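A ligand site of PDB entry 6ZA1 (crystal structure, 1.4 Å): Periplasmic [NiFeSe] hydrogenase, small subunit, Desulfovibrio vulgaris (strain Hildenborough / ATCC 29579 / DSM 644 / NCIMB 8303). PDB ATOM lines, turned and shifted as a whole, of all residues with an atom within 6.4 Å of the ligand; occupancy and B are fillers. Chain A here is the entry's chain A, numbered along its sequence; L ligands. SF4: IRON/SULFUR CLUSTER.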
ATOM      1  N   ILE A 207       0.867   6.861  14.364  1.00  0.00           N
ATOM      2  CA  ILE A 207       0.379   5.891  13.383  1.00  0.00           C
ATOM      3  C   ILE A 207       0.176   6.552  12.022  1.00  0.00           C
ATOM      4  O   ILE A 207       0.651   6.073  10.992  1.00  0.00           O
ATOM      5  CB  ILE A 207      -0.913   5.221  13.878  1.00  0.00           C
ATOM      6  CG1 ILE A 207      -0.607   4.325  15.070  1.00  0.00           C
ATOM      7  CG2 ILE A 207      -1.582   4.439  12.750  1.00  0.00           C
ATOM      8  CD1 ILE A 207      -1.636   3.266  15.362  1.00  0.00           C
ATOM      9  N   HIS A 208      -0.582   7.653  12.001  1.00  0.00           N
ATOM     10  CA  HIS A 208      -1.018   8.239  10.749  1.00  0.00           C
ATOM     11  C   HIS A 208       0.148   8.784   9.931  1.00  0.00           C
ATOM     12  O   HIS A 208       0.207   8.596   8.716  1.00  0.00           O
ATOM     13  CB  HIS A 208      -2.057   9.309  11.091  1.00  0.00           C
ATOM     14  CG  HIS A 208      -2.395  10.249   9.982  1.00  0.00           C
ATOM     15  ND1 HIS A 208      -3.329   9.943   9.009  1.00  0.00           N
ATOM     16  CD2 HIS A 208      -1.979  11.511   9.722  1.00  0.00           C
ATOM     17  CE1 HIS A 208      -3.451  10.969   8.192  1.00  0.00           C
ATOM     18  NE2 HIS A 208      -2.643  11.925   8.591  1.00  0.00           N
ATOM     19  N   GLU A 209       1.113   9.441  10.590  1.00  0.00           N
ATOM     20  CA  GLU A 209       2.231  10.014   9.848  1.00  0.00           C
ATOM     21  C   GLU A 209       3.095   8.932   9.197  1.00  0.00           C
ATOM     22  O   GLU A 209       3.869   9.244   8.287  1.00  0.00           O
ATOM     23  CB  GLU A 209       3.103  10.873  10.754  1.00  0.00           C
ATOM     24  CG  GLU A 209       2.393  12.086  11.319  1.00  0.00           C
ATOM     25  CD  GLU A 209       1.863  13.023  10.245  1.00  0.00           C
ATOM     26  OE1 GLU A 209       2.579  13.273   9.254  1.00  0.00           O
ATOM     27  OE2 GLU A 209       0.727  13.514  10.399  1.00  0.00           O
ATOM     28  N   CYS A 211       1.569   5.921   8.143  1.00  0.00           N
ATOM     29  CA  CYS A 211       0.576   4.968   7.662  1.00  0.00           C
ATOM     30  C   CYS A 211       0.752   4.708   6.171  1.00  0.00           C
ATOM     31  O   CYS A 211       0.947   5.653   5.388  1.00  0.00           O
ATOM     32  CB  CYS A 211      -0.824   5.502   7.912  1.00  0.00           C
ATOM     33  SG  CYS A 211      -2.114   4.356   7.357  1.00  0.00           S
ATOM     34  N   PRO A 212       0.656   3.450   5.739  1.00  0.00           N
ATOM     35  CA  PRO A 212       0.750   3.178   4.287  1.00  0.00           C
ATOM     36  C   PRO A 212      -0.351   3.822   3.468  1.00  0.00           C
ATOM     37  O   PRO A 212      -0.180   3.974   2.255  1.00  0.00           O
ATOM     38  CB  PRO A 212       0.707   1.639   4.204  1.00  0.00           C
ATOM     39  CG  PRO A 212       0.077   1.208   5.471  1.00  0.00           C
ATOM     40  CD  PRO A 212       0.488   2.213   6.514  1.00  0.00           C
ATOM     41  N   TYR A 213      -1.479   4.209   4.063  1.00  0.00           N
ATOM     42  CA  TYR A 213      -2.556   4.835   3.300  1.00  0.00           C
ATOM     43  C   TYR A 213      -2.491   6.353   3.339  1.00  0.00           C
ATOM     44  O   TYR A 213      -3.423   7.013   2.869  1.00  0.00           O
ATOM     45  CB  TYR A 213      -3.912   4.283   3.733  1.00  0.00           C
ATOM     46  CG  TYR A 213      -3.886   2.765   3.846  1.00  0.00           C
ATOM     47  CD1 TYR A 213      -3.801   1.956   2.708  1.00  0.00           C
ATOM     48  CD2 TYR A 213      -3.918   2.147   5.084  1.00  0.00           C
ATOM     49  CE1 TYR A 213      -3.765   0.568   2.813  1.00  0.00           C
ATOM     50  CE2 TYR A 213      -3.872   0.762   5.198  1.00  0.00           C
ATOM     51  CZ  TYR A 213      -3.790  -0.021   4.077  1.00  0.00           C
ATOM     52  OH  TYR A 213      -3.752  -1.393   4.209  1.00  0.00           O
ATOM     53  N   LEU A 214      -1.396   6.929   3.849  1.00  0.00           N
ATOM     54  CA  LEU A 214      -1.300   8.379   3.952  1.00  0.00           C
ATOM     55  C   LEU A 214      -1.398   9.066   2.591  1.00  0.00           C
ATOM     56  O   LEU A 214      -1.927  10.181   2.498  1.00  0.00           O
ATOM     57  CB  LEU A 214      -0.010   8.778   4.669  1.00  0.00           C
ATOM     58  CG  LEU A 214       0.163  10.250   5.086  1.00  0.00           C
ATOM     59  CD1 LEU A 214      -0.912  10.706   6.042  1.00  0.00           C
ATOM     60  CD2 LEU A 214       1.552  10.435   5.702  1.00  0.00           C
ATOM     61  N   ASP A 215      -0.893   8.427   1.528  1.00  0.00           N
ATOM     62  CA  ASP A 215      -1.040   9.006   0.194  1.00  0.00           C
ATOM     63  C   ASP A 215      -2.509   9.190  -0.165  1.00  0.00           C
ATOM     64  O   ASP A 215      -2.901  10.231  -0.717  1.00  0.00           O
ATOM     65  CB  ASP A 215      -0.299   8.160  -0.854  1.00  0.00           C
ATOM     66  CG  ASP A 215      -0.840   6.737  -0.998  1.00  0.00           C
ATOM     67  OD1 ASP A 215      -1.282   6.150   0.002  1.00  0.00           O
ATOM     68  OD2 ASP A 215      -0.789   6.208  -2.127  1.00  0.00           O
ATOM     69  N   LYS A 216      -3.360   8.210   0.169  1.00  0.00           N
ATOM     70  CA  LYS A 216      -4.781   8.326  -0.101  1.00  0.00           C
ATOM     71  C   LYS A 216      -5.423   9.414   0.744  1.00  0.00           C
ATOM     72  O   LYS A 216      -6.267  10.180   0.268  1.00  0.00           O
ATOM     73  CB  LYS A 216      -5.462   6.985   0.147  1.00  0.00           C
ATOM     74  CG  LYS A 216      -4.904   5.829  -0.674  1.00  0.00           C
ATOM     75  CD  LYS A 216      -5.026   6.118  -2.154  1.00  0.00           C
ATOM     76  CE  LYS A 216      -4.399   5.007  -2.984  1.00  0.00           C
ATOM     77  NZ  LYS A 216      -4.274   5.426  -4.412  1.00  0.00           N
ATOM     78  N   TYR A 217      -5.036   9.497   2.025  1.00  0.00           N
ATOM     79  CA  TYR A 217      -5.499  10.582   2.878  1.00  0.00           C
ATOM     80  C   TYR A 217      -5.193  11.930   2.241  1.00  0.00           C
ATOM     81  O   TYR A 217      -6.068  12.791   2.110  1.00  0.00           O
ATOM     82  CB  TYR A 217      -4.835  10.480   4.242  1.00  0.00           C
ATOM     83  CG  TYR A 217      -5.194  11.596   5.210  1.00  0.00           C
ATOM     84  CD1 TYR A 217      -6.287  11.469   6.065  1.00  0.00           C
ATOM     85  CD2 TYR A 217      -4.445  12.758   5.270  1.00  0.00           C
ATOM     86  CE1 TYR A 217      -6.616  12.471   6.951  1.00  0.00           C
ATOM     87  CE2 TYR A 217      -4.768  13.773   6.155  1.00  0.00           C
ATOM     88  CZ  TYR A 217      -5.854  13.625   6.985  1.00  0.00           C
ATOM     89  OH  TYR A 217      -6.183  14.627   7.871  1.00  0.00           O
ATOM     90  N   MET A 222     -11.150   8.350   0.113  1.00  0.00           N
ATOM     91  CA  MET A 222     -11.613   7.736   1.345  1.00  0.00           C
ATOM     92  C   MET A 222     -12.504   6.540   1.034  1.00  0.00           C
ATOM     93  O   MET A 222     -13.382   6.622   0.164  1.00  0.00           O
ATOM     94  CB  MET A 222     -12.468   8.709   2.169  1.00  0.00           C
ATOM     95  CG  MET A 222     -11.743   9.948   2.606  1.00  0.00           C
ATOM     96  SD  MET A 222     -10.495   9.533   3.825  1.00  0.00           S
ATOM     97  CE  MET A 222      -9.628  11.090   3.933  1.00  0.00           C
ATOM     98  N   GLY A 231      -8.847   2.899  -0.309  1.00  0.00           N
ATOM     99  CA  GLY A 231      -8.895   4.228   0.256  1.00  0.00           C
ATOM    100  C   GLY A 231      -8.375   4.321   1.681  1.00  0.00           C
ATOM    101  O   GLY A 231      -8.139   3.326   2.368  1.00  0.00           O
ATOM    102  N   CYS A 232      -8.196   5.569   2.127  1.00  0.00           N
ATOM    103  CA  CYS A 232      -7.934   5.863   3.519  1.00  0.00           C
ATOM    104  C   CYS A 232      -9.186   5.585   4.346  1.00  0.00           C
ATOM    105  O   CYS A 232     -10.313   5.685   3.852  1.00  0.00           O
ATOM    106  CB  CYS A 232      -7.483   7.316   3.673  1.00  0.00           C
ATOM    107  SG  CYS A 232      -7.506   8.030   5.333  1.00  0.00           S
ATOM    108  N   ARG A 233      -8.968   5.230   5.612  1.00  0.00           N
ATOM    109  CA  ARG A 233     -10.031   4.796   6.519  1.00  0.00           C
ATOM    110  C   ARG A 233     -10.561   5.924   7.407  1.00  0.00           C
ATOM    111  O   ARG A 233     -11.379   5.674   8.294  1.00  0.00           O
ATOM    112  CB  ARG A 233      -9.516   3.651   7.402  1.00  0.00           C
ATOM    113  CG  ARG A 233      -9.356   2.277   6.745  1.00  0.00           C
ATOM    114  CD  ARG A 233      -8.237   2.192   5.705  1.00  0.00           C
ATOM    115  NE  ARG A 233      -7.813   0.801   5.556  1.00  0.00           N
ATOM    116  CZ  ARG A 233      -7.365   0.229   4.440  1.00  0.00           C
ATOM    117  NH1 ARG A 233      -7.250   0.922   3.307  1.00  0.00           N
ATOM    118  NH2 ARG A 233      -7.013  -1.046   4.459  1.00  0.00           N
ATOM    119  N   TYR A 234     -10.136   7.166   7.165  1.00  0.00           N
ATOM    120  CA  TYR A 234     -10.510   8.262   8.053  1.00  0.00           C
ATOM    121  C   TYR A 234     -12.023   8.435   8.158  1.00  0.00           C
ATOM    122  O   TYR A 234     -12.554   8.628   9.259  1.00  0.00           O
ATOM    123  CB  TYR A 234      -9.886   9.549   7.534  1.00  0.00           C
ATOM    124  CG  TYR A 234     -10.147  10.761   8.383  1.00  0.00           C
ATOM    125  CD1 TYR A 234      -9.408  11.008   9.527  1.00  0.00           C
ATOM    126  CD2 TYR A 234     -11.133  11.669   8.039  1.00  0.00           C
ATOM    127  CE1 TYR A 234      -9.646  12.117  10.299  1.00  0.00           C
ATOM    128  CE2 TYR A 234     -11.378  12.781   8.794  1.00  0.00           C
ATOM    129  CZ  TYR A 234     -10.624  13.004   9.930  1.00  0.00           C
ATOM    130  OH  TYR A 234     -10.876  14.128  10.690  1.00  0.00           O
ATOM    131  N   ASP A 235     -12.728   8.402   7.028  1.00  0.00           N
ATOM    132  CA  ASP A 235     -14.171   8.639   7.071  1.00  0.00           C
ATOM    133  C   ASP A 235     -14.909   7.506   7.775  1.00  0.00           C
ATOM    134  O   ASP A 235     -16.027   7.708   8.265  1.00  0.00           O
ATOM    135  CB  ASP A 235     -14.728   8.820   5.663  1.00  0.00           C
ATOM    136  CG  ASP A 235     -14.474  10.222   5.119  1.00  0.00           C
ATOM    137  OD1 ASP A 235     -13.976  11.083   5.870  1.00  0.00           O
ATOM    138  OD2 ASP A 235     -14.785  10.455   3.941  1.00  0.00           O
ATOM    139  N   CYS A 238     -11.164   6.049  11.467  1.00  0.00           N
ATOM    140  CA  CYS A 238      -9.793   5.790  11.891  1.00  0.00           C
ATOM    141  C   CYS A 238      -9.259   6.901  12.782  1.00  0.00           C
ATOM    142  O   CYS A 238      -9.331   8.081  12.431  1.00  0.00           O
ATOM    143  CB  CYS A 238      -8.903   5.639  10.663  1.00  0.00           C
ATOM    144  SG  CYS A 238      -7.233   5.132  11.082  1.00  0.00           S
ATOM    145  N   LYS A 239      -8.718   6.502  13.934  1.00  0.00           N
ATOM    146  CA  LYS A 239      -8.133   7.431  14.900  1.00  0.00           C
ATOM    147  C   LYS A 239      -6.611   7.455  14.836  1.00  0.00           C
ATOM    148  O   LYS A 239      -5.963   7.983  15.749  1.00  0.00           O
ATOM    149  CB  LYS A 239      -8.612   7.072  16.312  1.00  0.00           C
ATOM    150  CG  LYS A 239     -10.134   7.068  16.474  1.00  0.00           C
ATOM    151  CD  LYS A 239     -10.748   8.393  16.015  1.00  0.00           C
ATOM    152  CE  LYS A 239     -12.211   8.530  16.429  1.00  0.00           C
ATOM    153  NZ  LYS A 239     -13.079   7.491  15.806  1.00  0.00           N
ATOM    154  N   GLY A 240      -6.019   6.899  13.777  1.00  0.00           N
ATOM    155  CA  GLY A 240      -4.590   6.955  13.586  1.00  0.00           C
ATOM    156  C   GLY A 240      -3.968   8.322  13.750  1.00  0.00           C
ATOM    157  O   GLY A 240      -2.850   8.427  14.281  1.00  0.00           O
ATOM    158  N   PRO A 241      -4.627   9.400  13.301  1.00  0.00           N
ATOM    159  CA  PRO A 241      -4.031  10.740  13.471  1.00  0.00           C
ATOM    160  C   PRO A 241      -3.710  11.102  14.908  1.00  0.00           C
ATOM    161  O   PRO A 241      -2.766  11.871  15.152  1.00  0.00           O
ATOM    162  CB  PRO A 241      -5.081  11.677  12.875  1.00  0.00           C
ATOM    163  CG  PRO A 241      -5.778  10.843  11.857  1.00  0.00           C
ATOM    164  CD  PRO A 241      -5.825   9.440  12.441  1.00  0.00           C
ATOM    165  N   TRP A 258      -3.161  -5.917  10.805  1.00  0.00           N
ATOM    166  CA  TRP A 258      -3.258  -4.883  11.841  1.00  0.00           C
ATOM    167  C   TRP A 258      -4.568  -4.136  11.666  1.00  0.00           C
ATOM    168  O   TRP A 258      -5.273  -4.290  10.668  1.00  0.00           O
ATOM    169  CB  TRP A 258      -2.048  -3.958  11.862  1.00  0.00           C
ATOM    170  CG  TRP A 258      -1.853  -3.054  10.687  1.00  0.00           C
ATOM    171  CD1 TRP A 258      -1.668  -3.414   9.392  1.00  0.00           C
ATOM    172  CD2 TRP A 258      -1.741  -1.624  10.731  1.00  0.00           C
ATOM    173  NE1 TRP A 258      -1.479  -2.298   8.607  1.00  0.00           N
ATOM    174  CE2 TRP A 258      -1.506  -1.184   9.413  1.00  0.00           C
ATOM    175  CE3 TRP A 258      -1.818  -0.673  11.744  1.00  0.00           C
ATOM    176  CZ2 TRP A 258      -1.365   0.160   9.089  1.00  0.00           C
ATOM    177  CZ3 TRP A 258      -1.673   0.661  11.430  1.00  0.00           C
ATOM    178  CH2 TRP A 258      -1.452   1.068  10.106  1.00  0.00           C
ATOM    179  N   VAL A 260      -5.634  -1.062  11.066  1.00  0.00           N
ATOM    180  CA  VAL A 260      -5.941  -0.144   9.973  1.00  0.00           C
ATOM    181  C   VAL A 260      -6.151  -0.906   8.679  1.00  0.00           C
ATOM    182  O   VAL A 260      -7.043  -0.567   7.882  1.00  0.00           O
ATOM    183  CB  VAL A 260      -4.847   0.937   9.847  1.00  0.00           C
ATOM    184  CG1 VAL A 260      -5.078   1.753   8.599  1.00  0.00           C
ATOM    185  CG2 VAL A 260      -4.846   1.826  11.084  1.00  0.00           C
ATOM    186  N   CYS A 265      -8.163   2.006  13.160  1.00  0.00           N
ATOM    187  CA  CYS A 265      -7.543   2.178  14.467  1.00  0.00           C
ATOM    188  C   CYS A 265      -8.524   2.894  15.384  1.00  0.00           C
ATOM    189  O   CYS A 265      -9.182   3.854  14.972  1.00  0.00           O
ATOM    190  CB  CYS A 265      -6.265   3.006  14.332  1.00  0.00           C
ATOM    191  SG  CYS A 265      -5.414   3.467  15.857  1.00  0.00           S
HETATM  192 FE1  SF4 L   1      -6.047   6.077   9.356  1.00  0.00          FE
HETATM  193 FE2  SF4 L   1      -4.350   8.154   8.717  1.00  0.00          FE
HETATM  194 FE3  SF4 L   1      -5.995   7.207   6.807  1.00  0.00          FE
HETATM  195 FE4  SF4 L   1      -3.865   5.726   7.730  1.00  0.00          FE
HETATM  196  S1  SF4 L   1      -3.768   7.680   6.534  1.00  0.00           S
HETATM  197  S2  SF4 L   1      -6.016   4.977   7.315  1.00  0.00           S
HETATM  198  S3  SF4 L   1      -3.848   6.303   9.963  1.00  0.00           S
HETATM  199  S4  SF4 L   1      -6.651   8.195   8.789  1.00  0.00           S
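The backbone NH (N) of His 208 lies within hydrogen-bond range of the backbone carbonyl oxygen (O) of Gly 240. SG of Cys 211 lies close to N of Tyr 213 (3.4 Å). The side-chain sulfur of Cys 232 lies close to the backbone NH of Tyr 234 (3.3 Å). SG of Cys 232 lies close to SD of Met 222, at 3.7 Å. The backbone NH (N) of Cys 238 is in hydrogen-bond range of the backbone carbonyl oxygen (O) of Arg 233 (3.2 Å). The side-chain sulfur of Cys 238 lies close to the backbone NH of Gly 240. NE of Arg 233 sits at hydrogen-bond distance from O of Val 260, 2.8 Å away. The guanidinium group (NH2) of Arg 233 sits at hydrogen-bond distance from the side-chain hydroxyl (OH) of Tyr 213 (3.3 Å).
ND1 of His 208 is bound to FE2 of the ligand (2.1 Å). SG of Cys 211 is bound to FE4 of the ligand, 2.3 Å away. The side-chain sulfur of Cys 232 binds an iron atom (FE3) of the ligand, 2.3 Å away. SG of Cys 238 is bound to FE1 of the ligand (2.3 Å). N of Arg 233 sits close to S2 of the ligand, 3.4 Å away. A sulfur (S1) of the ligand lies close to the backbone NH (N) of Leu 214, 3.7 Å away.
S1 of the ligand lies close to O of Tyr 213 (3.7 Å). Tyr 217 touches the ligand (CB to S1, 3.8 Å). CB of Tyr 234 touches S4 of the ligand, at 3.7 Å. Gly 240 touches the ligand (CA to S3, 3.8 Å). Pro 241 touches the ligand (CD to S4, 3.9 Å). Val 260 touches the ligand (CG1 to S2, 3.6 Å). Hydrophobic or aromatic side chains that line the ligand: His 208, Tyr 217, Tyr 234, Pro 241 and Val 260. Within 4 Å of the ligand: His 208, Cys 211, Tyr 213, Leu 214, Tyr 217, Cys 232, Arg 233, Tyr 234, Cys 238, Gly 240, Pro 241 and Val 260. The nearest printed residue that does not touch the ligand is Ile 207 (4.05 Å).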
